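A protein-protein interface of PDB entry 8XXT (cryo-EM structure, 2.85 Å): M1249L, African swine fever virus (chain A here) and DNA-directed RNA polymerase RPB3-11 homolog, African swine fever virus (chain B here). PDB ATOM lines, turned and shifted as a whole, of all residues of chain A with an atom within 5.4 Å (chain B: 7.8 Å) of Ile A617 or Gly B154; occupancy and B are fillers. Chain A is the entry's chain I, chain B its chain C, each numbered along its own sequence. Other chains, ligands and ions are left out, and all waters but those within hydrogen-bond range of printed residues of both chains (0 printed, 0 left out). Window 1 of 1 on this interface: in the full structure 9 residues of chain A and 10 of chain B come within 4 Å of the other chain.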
ATOM      1  N   ALA A 612     -15.065  -3.269 -21.650  1.00  0.00           N
ATOM      2  CA  ALA A 612     -16.308  -3.586 -20.958  1.00  0.00           C
ATOM      3  C   ALA A 612     -17.516  -3.372 -21.861  1.00  0.00           C
ATOM      4  O   ALA A 612     -18.406  -4.226 -21.924  1.00  0.00           O
ATOM      5  CB  ALA A 612     -16.434  -2.747 -19.687  1.00  0.00           C
ATOM      6  N   THR A 613     -17.557  -2.248 -22.584  1.00  0.00           N
ATOM      7  CA  THR A 613     -18.739  -1.926 -23.375  1.00  0.00           C
ATOM      8  C   THR A 613     -18.924  -2.887 -24.543  1.00  0.00           C
ATOM      9  O   THR A 613     -20.050  -3.066 -25.020  1.00  0.00           O
ATOM     10  CB  THR A 613     -18.673  -0.480 -23.873  1.00  0.00           C
ATOM     11  OG1 THR A 613     -19.999   0.010 -24.099  1.00  0.00           O
ATOM     12  CG2 THR A 613     -17.878  -0.375 -25.166  1.00  0.00           C
ATOM     13  N   VAL A 614     -17.848  -3.520 -25.012  1.00  0.00           N
ATOM     14  CA  VAL A 614     -17.995  -4.492 -26.089  1.00  0.00           C
ATOM     15  C   VAL A 614     -18.349  -5.863 -25.525  1.00  0.00           C
ATOM     16  O   VAL A 614     -18.913  -6.702 -26.234  1.00  0.00           O
ATOM     17  CB  VAL A 614     -16.724  -4.541 -26.953  1.00  0.00           C
ATOM     18  CG1 VAL A 614     -15.711  -5.501 -26.361  1.00  0.00           C
ATOM     19  CG2 VAL A 614     -17.067  -4.926 -28.380  1.00  0.00           C
ATOM     20  N   ALA A 615     -18.024  -6.116 -24.256  1.00  0.00           N
ATOM     21  CA  ALA A 615     -18.498  -7.331 -23.605  1.00  0.00           C
ATOM     22  C   ALA A 615     -19.982  -7.238 -23.285  1.00  0.00           C
ATOM     23  O   ALA A 615     -20.691  -8.249 -23.332  1.00  0.00           O
ATOM     24  CB  ALA A 615     -17.692  -7.599 -22.335  1.00  0.00           C
ATOM     25  N   ARG A 616     -20.464  -6.039 -22.950  1.00  0.00           N
ATOM     26  CA  ARG A 616     -21.890  -5.850 -22.710  1.00  0.00           C
ATOM     27  C   ARG A 616     -22.693  -6.052 -23.987  1.00  0.00           C
ATOM     28  O   ARG A 616     -23.779  -6.644 -23.957  1.00  0.00           O
ATOM     29  CB  ARG A 616     -22.137  -4.458 -22.129  1.00  0.00           C
ATOM     30  CG  ARG A 616     -21.304  -4.177 -20.896  1.00  0.00           C
ATOM     31  CD  ARG A 616     -21.954  -3.193 -19.954  1.00  0.00           C
ATOM     32  NE  ARG A 616     -21.836  -3.648 -18.574  1.00  0.00           N
ATOM     33  CZ  ARG A 616     -20.920  -3.216 -17.717  1.00  0.00           C
ATOM     34  NH1 ARG A 616     -20.028  -2.304 -18.062  1.00  0.00           N
ATOM     35  NH2 ARG A 616     -20.897  -3.718 -16.487  1.00  0.00           N
ATOM     36  N   ILE A 617     -22.172  -5.570 -25.118  1.00  0.00           N
ATOM     37  CA  ILE A 617     -22.859  -5.749 -26.395  1.00  0.00           C
ATOM     38  C   ILE A 617     -22.991  -7.230 -26.718  1.00  0.00           C
ATOM     39  O   ILE A 617     -24.065  -7.712 -27.094  1.00  0.00           O
ATOM     40  CB  ILE A 617     -22.114  -4.997 -27.510  1.00  0.00           C
ATOM     41  CG1 ILE A 617     -22.324  -3.493 -27.369  1.00  0.00           C
ATOM     42  CG2 ILE A 617     -22.566  -5.482 -28.876  1.00  0.00           C
ATOM     43  CD1 ILE A 617     -21.316  -2.683 -28.125  1.00  0.00           C
ATOM     44  N   ASP A 618     -21.895  -7.976 -26.571  1.00  0.00           N
ATOM     45  CA  ASP A 618     -21.935  -9.416 -26.784  1.00  0.00           C
ATOM     46  C   ASP A 618     -22.691 -10.133 -25.673  1.00  0.00           C
ATOM     47  O   ASP A 618     -23.149 -11.264 -25.875  1.00  0.00           O
ATOM     48  CB  ASP A 618     -20.506  -9.952 -26.912  1.00  0.00           C
ATOM     49  CG  ASP A 618     -20.410 -11.445 -26.666  1.00  0.00           C
ATOM     50  OD1 ASP A 618     -20.586 -12.222 -27.627  1.00  0.00           O
ATOM     51  OD2 ASP A 618     -20.153 -11.841 -25.509  1.00  0.00           O
ATOM     52  N   GLY A 619     -22.864  -9.493 -24.520  1.00  0.00           N
ATOM     53  CA  GLY A 619     -23.528 -10.129 -23.405  1.00  0.00           C
ATOM     54  C   GLY A 619     -22.641 -10.998 -22.549  1.00  0.00           C
ATOM     55  O   GLY A 619     -23.156 -11.734 -21.699  1.00  0.00           O
ATOM     56  N   MET A 623     -25.099  -6.359 -17.858  1.00  0.00           N
ATOM     57  CA  MET A 623     -25.164  -4.994 -18.367  1.00  0.00           C
ATOM     58  C   MET A 623     -24.750  -3.984 -17.304  1.00  0.00           C
ATOM     59  O   MET A 623     -23.952  -3.081 -17.577  1.00  0.00           O
ATOM     60  CB  MET A 623     -26.572  -4.691 -18.878  1.00  0.00           C
ATOM     61  CG  MET A 623     -26.647  -3.480 -19.790  1.00  0.00           C
ATOM     62  SD  MET A 623     -26.247  -3.888 -21.501  1.00  0.00           S
ATOM     63  CE  MET A 623     -27.174  -2.632 -22.373  1.00  0.00           C
ATOM     64  N   TYR A 699     -17.998  -0.771 -36.210  1.00  0.00           N
ATOM     65  CA  TYR A 699     -17.768  -0.668 -34.773  1.00  0.00           C
ATOM     66  C   TYR A 699     -16.864  -1.788 -34.279  1.00  0.00           C
ATOM     67  O   TYR A 699     -15.846  -1.535 -33.625  1.00  0.00           O
ATOM     68  CB  TYR A 699     -19.103  -0.686 -34.032  1.00  0.00           C
ATOM     69  CG  TYR A 699     -18.980  -0.497 -32.539  1.00  0.00           C
ATOM     70  CD1 TYR A 699     -18.713   0.753 -31.994  1.00  0.00           C
ATOM     71  CD2 TYR A 699     -19.148  -1.566 -31.671  1.00  0.00           C
ATOM     72  CE1 TYR A 699     -18.606   0.926 -30.627  1.00  0.00           C
ATOM     73  CE2 TYR A 699     -19.040  -1.403 -30.311  1.00  0.00           C
ATOM     74  CZ  TYR A 699     -18.772  -0.156 -29.792  1.00  0.00           C
ATOM     75  OH  TYR A 699     -18.667   0.002 -28.430  1.00  0.00           O
ATOM     76  N   SER B  82     -24.645   1.298 -15.521  1.00  0.00           N
ATOM     77  CA  SER B  82     -24.655   0.917 -16.925  1.00  0.00           C
ATOM     78  C   SER B  82     -25.385   1.915 -17.800  1.00  0.00           C
ATOM     79  O   SER B  82     -25.278   1.834 -19.029  1.00  0.00           O
ATOM     80  CB  SER B  82     -25.319  -0.446 -17.101  1.00  0.00           C
ATOM     81  OG  SER B  82     -25.186  -0.906 -18.434  1.00  0.00           O
ATOM     82  N   THR B  83     -26.123   2.842 -17.197  1.00  0.00           N
ATOM     83  CA  THR B  83     -26.974   3.739 -17.959  1.00  0.00           C
ATOM     84  C   THR B  83     -26.143   4.583 -18.916  1.00  0.00           C
ATOM     85  O   THR B  83     -24.953   4.821 -18.699  1.00  0.00           O
ATOM     86  CB  THR B  83     -27.772   4.638 -17.016  1.00  0.00           C
ATOM     87  OG1 THR B  83     -26.873   5.361 -16.167  1.00  0.00           O
ATOM     88  CG2 THR B  83     -28.705   3.802 -16.159  1.00  0.00           C
ATOM     89  N   ASP B  84     -26.778   5.009 -20.004  1.00  0.00           N
ATOM     90  CA  ASP B  84     -26.080   5.812 -20.994  1.00  0.00           C
ATOM     91  C   ASP B  84     -25.555   7.086 -20.358  1.00  0.00           C
ATOM     92  O   ASP B  84     -26.279   7.788 -19.649  1.00  0.00           O
ATOM     93  CB  ASP B  84     -27.000   6.149 -22.163  1.00  0.00           C
ATOM     94  CG  ASP B  84     -26.246   6.729 -23.338  1.00  0.00           C
ATOM     95  OD1 ASP B  84     -25.001   6.636 -23.343  1.00  0.00           O
ATOM     96  OD2 ASP B  84     -26.890   7.278 -24.255  1.00  0.00           O
ATOM     97  N   LEU B 115     -32.505  -1.271 -23.372  1.00  0.00           N
ATOM     98  CA  LEU B 115     -31.128  -1.739 -23.413  1.00  0.00           C
ATOM     99  C   LEU B 115     -30.664  -1.782 -24.859  1.00  0.00           C
ATOM    100  O   LEU B 115     -31.424  -2.173 -25.751  1.00  0.00           O
ATOM    101  CB  LEU B 115     -30.997  -3.127 -22.781  1.00  0.00           C
ATOM    102  CG  LEU B 115     -30.795  -3.232 -21.267  1.00  0.00           C
ATOM    103  CD1 LEU B 115     -31.987  -2.689 -20.497  1.00  0.00           C
ATOM    104  CD2 LEU B 115     -30.526  -4.678 -20.877  1.00  0.00           C
ATOM    105  N   ASN B 116     -29.423  -1.376 -25.094  1.00  0.00           N
ATOM    106  CA  ASN B 116     -28.830  -1.400 -26.427  1.00  0.00           C
ATOM    107  C   ASN B 116     -27.790  -2.517 -26.450  1.00  0.00           C
ATOM    108  O   ASN B 116     -26.614  -2.297 -26.158  1.00  0.00           O
ATOM    109  CB  ASN B 116     -28.216  -0.056 -26.782  1.00  0.00           C
ATOM    110  CG  ASN B 116     -27.886   0.060 -28.249  1.00  0.00           C
ATOM    111  OD1 ASN B 116     -28.187  -0.834 -29.034  1.00  0.00           O
ATOM    112  ND2 ASN B 116     -27.269   1.167 -28.631  1.00  0.00           N
ATOM    113  N   ASN B 117     -28.236  -3.723 -26.797  1.00  0.00           N
ATOM    114  CA  ASN B 117     -27.369  -4.889 -26.883  1.00  0.00           C
ATOM    115  C   ASN B 117     -26.713  -5.031 -28.247  1.00  0.00           C
ATOM    116  O   ASN B 117     -26.295  -6.137 -28.610  1.00  0.00           O
ATOM    117  CB  ASN B 117     -28.155  -6.160 -26.557  1.00  0.00           C
ATOM    118  CG  ASN B 117     -28.446  -6.301 -25.081  1.00  0.00           C
ATOM    119  OD1 ASN B 117     -29.594  -6.204 -24.650  1.00  0.00           O
ATOM    120  ND2 ASN B 117     -27.404  -6.535 -24.296  1.00  0.00           N
ATOM    121  N   SER B 118     -26.610  -3.947 -29.006  1.00  0.00           N
ATOM    122  CA  SER B 118     -26.109  -4.008 -30.368  1.00  0.00           C
ATOM    123  C   SER B 118     -25.047  -2.938 -30.568  1.00  0.00           C
ATOM    124  O   SER B 118     -24.747  -2.148 -29.670  1.00  0.00           O
ATOM    125  CB  SER B 118     -27.247  -3.846 -31.376  1.00  0.00           C
ATOM    126  OG  SER B 118     -27.971  -2.654 -31.131  1.00  0.00           O
ATOM    127  N   CYS B 119     -24.473  -2.923 -31.767  1.00  0.00           N
ATOM    128  CA  CYS B 119     -23.378  -2.024 -32.093  1.00  0.00           C
ATOM    129  C   CYS B 119     -23.842  -0.685 -32.647  1.00  0.00           C
ATOM    130  O   CYS B 119     -22.999   0.174 -32.928  1.00  0.00           O
ATOM    131  CB  CYS B 119     -22.435  -2.686 -33.100  1.00  0.00           C
ATOM    132  SG  CYS B 119     -21.456  -4.034 -32.413  1.00  0.00           S
ATOM    133  N   GLU B 120     -25.142  -0.482 -32.814  1.00  0.00           N
ATOM    134  CA  GLU B 120     -25.662   0.772 -33.335  1.00  0.00           C
ATOM    135  C   GLU B 120     -26.238   1.619 -32.210  1.00  0.00           C
ATOM    136  O   GLU B 120     -26.526   1.132 -31.115  1.00  0.00           O
ATOM    137  CB  GLU B 120     -26.732   0.523 -34.399  1.00  0.00           C
ATOM    138  CG  GLU B 120     -28.150   0.447 -33.848  1.00  0.00           C
ATOM    139  CD  GLU B 120     -28.619  -0.975 -33.633  1.00  0.00           C
ATOM    140  OE1 GLU B 120     -27.785  -1.895 -33.748  1.00  0.00           O
ATOM    141  OE2 GLU B 120     -29.817  -1.174 -33.342  1.00  0.00           O
ATOM    142  N   VAL B 121     -26.403   2.905 -32.498  1.00  0.00           N
ATOM    143  CA  VAL B 121     -27.049   3.820 -31.565  1.00  0.00           C
ATOM    144  C   VAL B 121     -28.551   3.575 -31.620  1.00  0.00           C
ATOM    145  O   VAL B 121     -29.197   3.838 -32.639  1.00  0.00           O
ATOM    146  CB  VAL B 121     -26.714   5.279 -31.897  1.00  0.00           C
ATOM    147  CG1 VAL B 121     -27.473   6.213 -30.983  1.00  0.00           C
ATOM    148  CG2 VAL B 121     -25.220   5.517 -31.780  1.00  0.00           C
ATOM    149  N   LYS B 122     -29.109   3.068 -30.525  1.00  0.00           N
ATOM    150  CA  LYS B 122     -30.527   2.747 -30.450  1.00  0.00           C
ATOM    151  C   LYS B 122     -31.283   3.951 -29.908  1.00  0.00           C
ATOM    152  O   LYS B 122     -30.929   4.491 -28.857  1.00  0.00           O
ATOM    153  CB  LYS B 122     -30.754   1.527 -29.561  1.00  0.00           C
ATOM    154  CG  LYS B 122     -32.203   1.281 -29.187  1.00  0.00           C
ATOM    155  CD  LYS B 122     -32.332   0.016 -28.361  1.00  0.00           C
ATOM    156  CE  LYS B 122     -33.740  -0.158 -27.822  1.00  0.00           C
ATOM    157  NZ  LYS B 122     -33.909  -1.465 -27.127  1.00  0.00           N
ATOM    158  N   LEU B 151     -29.471   5.672 -27.177  1.00  0.00           N
ATOM    159  CA  LEU B 151     -28.577   4.869 -26.354  1.00  0.00           C
ATOM    160  C   LEU B 151     -27.334   4.504 -27.150  1.00  0.00           C
ATOM    161  O   LEU B 151     -27.435   3.940 -28.244  1.00  0.00           O
ATOM    162  CB  LEU B 151     -29.275   3.604 -25.860  1.00  0.00           C
ATOM    163  CG  LEU B 151     -30.421   3.829 -24.881  1.00  0.00           C
ATOM    164  CD1 LEU B 151     -31.117   2.522 -24.563  1.00  0.00           C
ATOM    165  CD2 LEU B 151     -29.908   4.483 -23.619  1.00  0.00           C
ATOM    166  N   GLN B 152     -26.169   4.823 -26.598  1.00  0.00           N
ATOM    167  CA  GLN B 152     -24.918   4.414 -27.203  1.00  0.00           C
ATOM    168  C   GLN B 152     -24.771   2.900 -27.097  1.00  0.00           C
ATOM    169  O   GLN B 152     -25.390   2.271 -26.237  1.00  0.00           O
ATOM    170  CB  GLN B 152     -23.751   5.124 -26.523  1.00  0.00           C
ATOM    171  CG  GLN B 152     -23.741   6.621 -26.744  1.00  0.00           C
ATOM    172  CD  GLN B 152     -23.723   6.988 -28.212  1.00  0.00           C
ATOM    173  OE1 GLN B 152     -23.014   6.377 -29.009  1.00  0.00           O
ATOM    174  NE2 GLN B 152     -24.513   7.986 -28.581  1.00  0.00           N
ATOM    175  N   PRO B 153     -23.978   2.288 -27.976  1.00  0.00           N
ATOM    176  CA  PRO B 153     -23.877   0.823 -27.976  1.00  0.00           C
ATOM    177  C   PRO B 153     -23.449   0.291 -26.617  1.00  0.00           C
ATOM    178  O   PRO B 153     -22.505   0.790 -26.004  1.00  0.00           O
ATOM    179  CB  PRO B 153     -22.819   0.545 -29.048  1.00  0.00           C
ATOM    180  CG  PRO B 153     -22.869   1.728 -29.939  1.00  0.00           C
ATOM    181  CD  PRO B 153     -23.185   2.892 -29.060  1.00  0.00           C
ATOM    182  N   GLY B 154     -24.159  -0.729 -26.148  1.00  0.00           N
ATOM    183  CA  GLY B 154     -23.869  -1.333 -24.868  1.00  0.00           C
ATOM    184  C   GLY B 154     -24.424  -0.600 -23.669  1.00  0.00           C
ATOM    185  O   GLY B 154     -24.260  -1.081 -22.542  1.00  0.00           O
ATOM    186  N   LYS B 155     -25.079   0.535 -23.869  1.00  0.00           N
ATOM    187  CA  LYS B 155     -25.618   1.337 -22.784  1.00  0.00           C
ATOM    188  C   LYS B 155     -27.119   1.117 -22.654  1.00  0.00           C
ATOM    189  O   LYS B 155     -27.788   0.662 -23.582  1.00  0.00           O
ATOM    190  CB  LYS B 155     -25.325   2.819 -23.014  1.00  0.00           C
ATOM    191  CG  LYS B 155     -23.852   3.141 -23.163  1.00  0.00           C
ATOM    192  CD  LYS B 155     -23.069   2.695 -21.944  1.00  0.00           C
ATOM    193  CE  LYS B 155     -21.639   3.192 -21.998  1.00  0.00           C
ATOM    194  NZ  LYS B 155     -20.854   2.729 -20.826  1.00  0.00           N
ATOM    195  N   SER B 156     -27.645   1.450 -21.479  1.00  0.00           N
ATOM    196  CA  SER B 156     -29.052   1.251 -21.172  1.00  0.00           C
ATOM    197  C   SER B 156     -29.621   2.521 -20.552  1.00  0.00           C
ATOM    198  O   SER B 156     -28.929   3.528 -20.393  1.00  0.00           O
ATOM    199  CB  SER B 156     -29.246   0.052 -20.236  1.00  0.00           C
ATOM    200  OG  SER B 156     -28.756   0.333 -18.940  1.00  0.00           O
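O of Ser B82 sits at hydrogen-bond distance from N of Ser B156, at 3.4 Å.
The backbone carbonyl oxygen (O) of Leu B115 lies within hydrogen-bond range of the side-chain amino group (NZ) of Lys B122.
O of Glu B120 lies within hydrogen-bond range of ND2 of Asn B116 (2.6 Å).
N of Gly B154 lies within hydrogen-bond range of O of Asn B116, at 2.9 Å.
N of Asn B116 lies within hydrogen-bond range of O of Lys B155.
OG of Ser B118 is in hydrogen-bond range of OE1 of Glu B120, 2.7 Å away.
OG of Ser B82 is in hydrogen-bond range of O of Met A623 (2.6 Å).
The backbone carbonyl oxygen (O) of Pro B153 sits at hydrogen-bond distance from the side-chain hydroxyl (OG1) of Thr A613 (3.2 Å).
The backbone carbonyl oxygen (O) of Ile A617 lies close to the backbone carbonyl oxygen (O) of Asn B117 (3.1 Å).
The side-chain sulfur (SD) of Met A623 sits close to the backbone carbonyl oxygen (O) of Gly B154 (3.6 Å).
Hydrophobic or aromatic side chains of chain A that line the printed part of chain B: Ile A617, Met A623 and Tyr A699.
Of the 17 printed residues of chain B, 9 touch a printed residue of chain A.
Printed residues of chain B that touch a printed residue of chain A: Ser B82, Leu B115, Asn B116, Asn B117, Ser B118, Cys B119, Pro B153, Gly B154 and Lys B155.
Among the printed residues, 13 pairs touch across the chains.
Among the printed residues, no Asp or Glu carboxylate lies within 4 Å of a Lys or Arg side-chain nitrogen of the other chain.
Asn B117 touches Arg A616 (ND2 to O, 3.6 Å).
Ser B118 touches Ile A617.
Ile A617 touches Cys B119 (CG2 to SG, 3.98 Å).
CD1 of Ile A617 touches CB of Pro B153, 3.7 Å away.
Gly B154 touches Ile A617 (N to CG1, 3.5 Å).
Leu B115 touches Met A623 (CG to CE, 3.8 Å).
Met A623 touches Asn B116.
Met A623 touches Lys B155 (CE to O, 3.6 Å).
Tyr A699 touches Cys B119.
Printed residues of chain B within 4 Å of Thr A613: Pro B153.
Of the printed residues of chain B, Ile A617 touches Asn B117, Ser B118, Cys B119, Pro B153 and Gly B154.
Printed residues of chain A within 4 Å of Ser B82: Met A623.
Of the printed residues of chain A, Asn B116 touches Met A623.
Printed residues of chain A within 4 Å of Asn B117: Arg A616 (3.6 Å) and Ile A617 (3.1 Å).
Of the printed residues of chain A, Cys B119 touches Ile A617 and Tyr A699.
Val B121 touches none of the printed residues of chain A.
Lys B122 touches none of the printed residues of chain A.
Of the printed residues of chain A, Gly B154 touches Ile A617 and Met A623.
The nearest residue of chain B that does not touch Ile A617 is Asn B116 (4.6 Å).
The nearest printed residue of chain A that does not touch Ser B82 is Arg A616 (4.2 Å).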
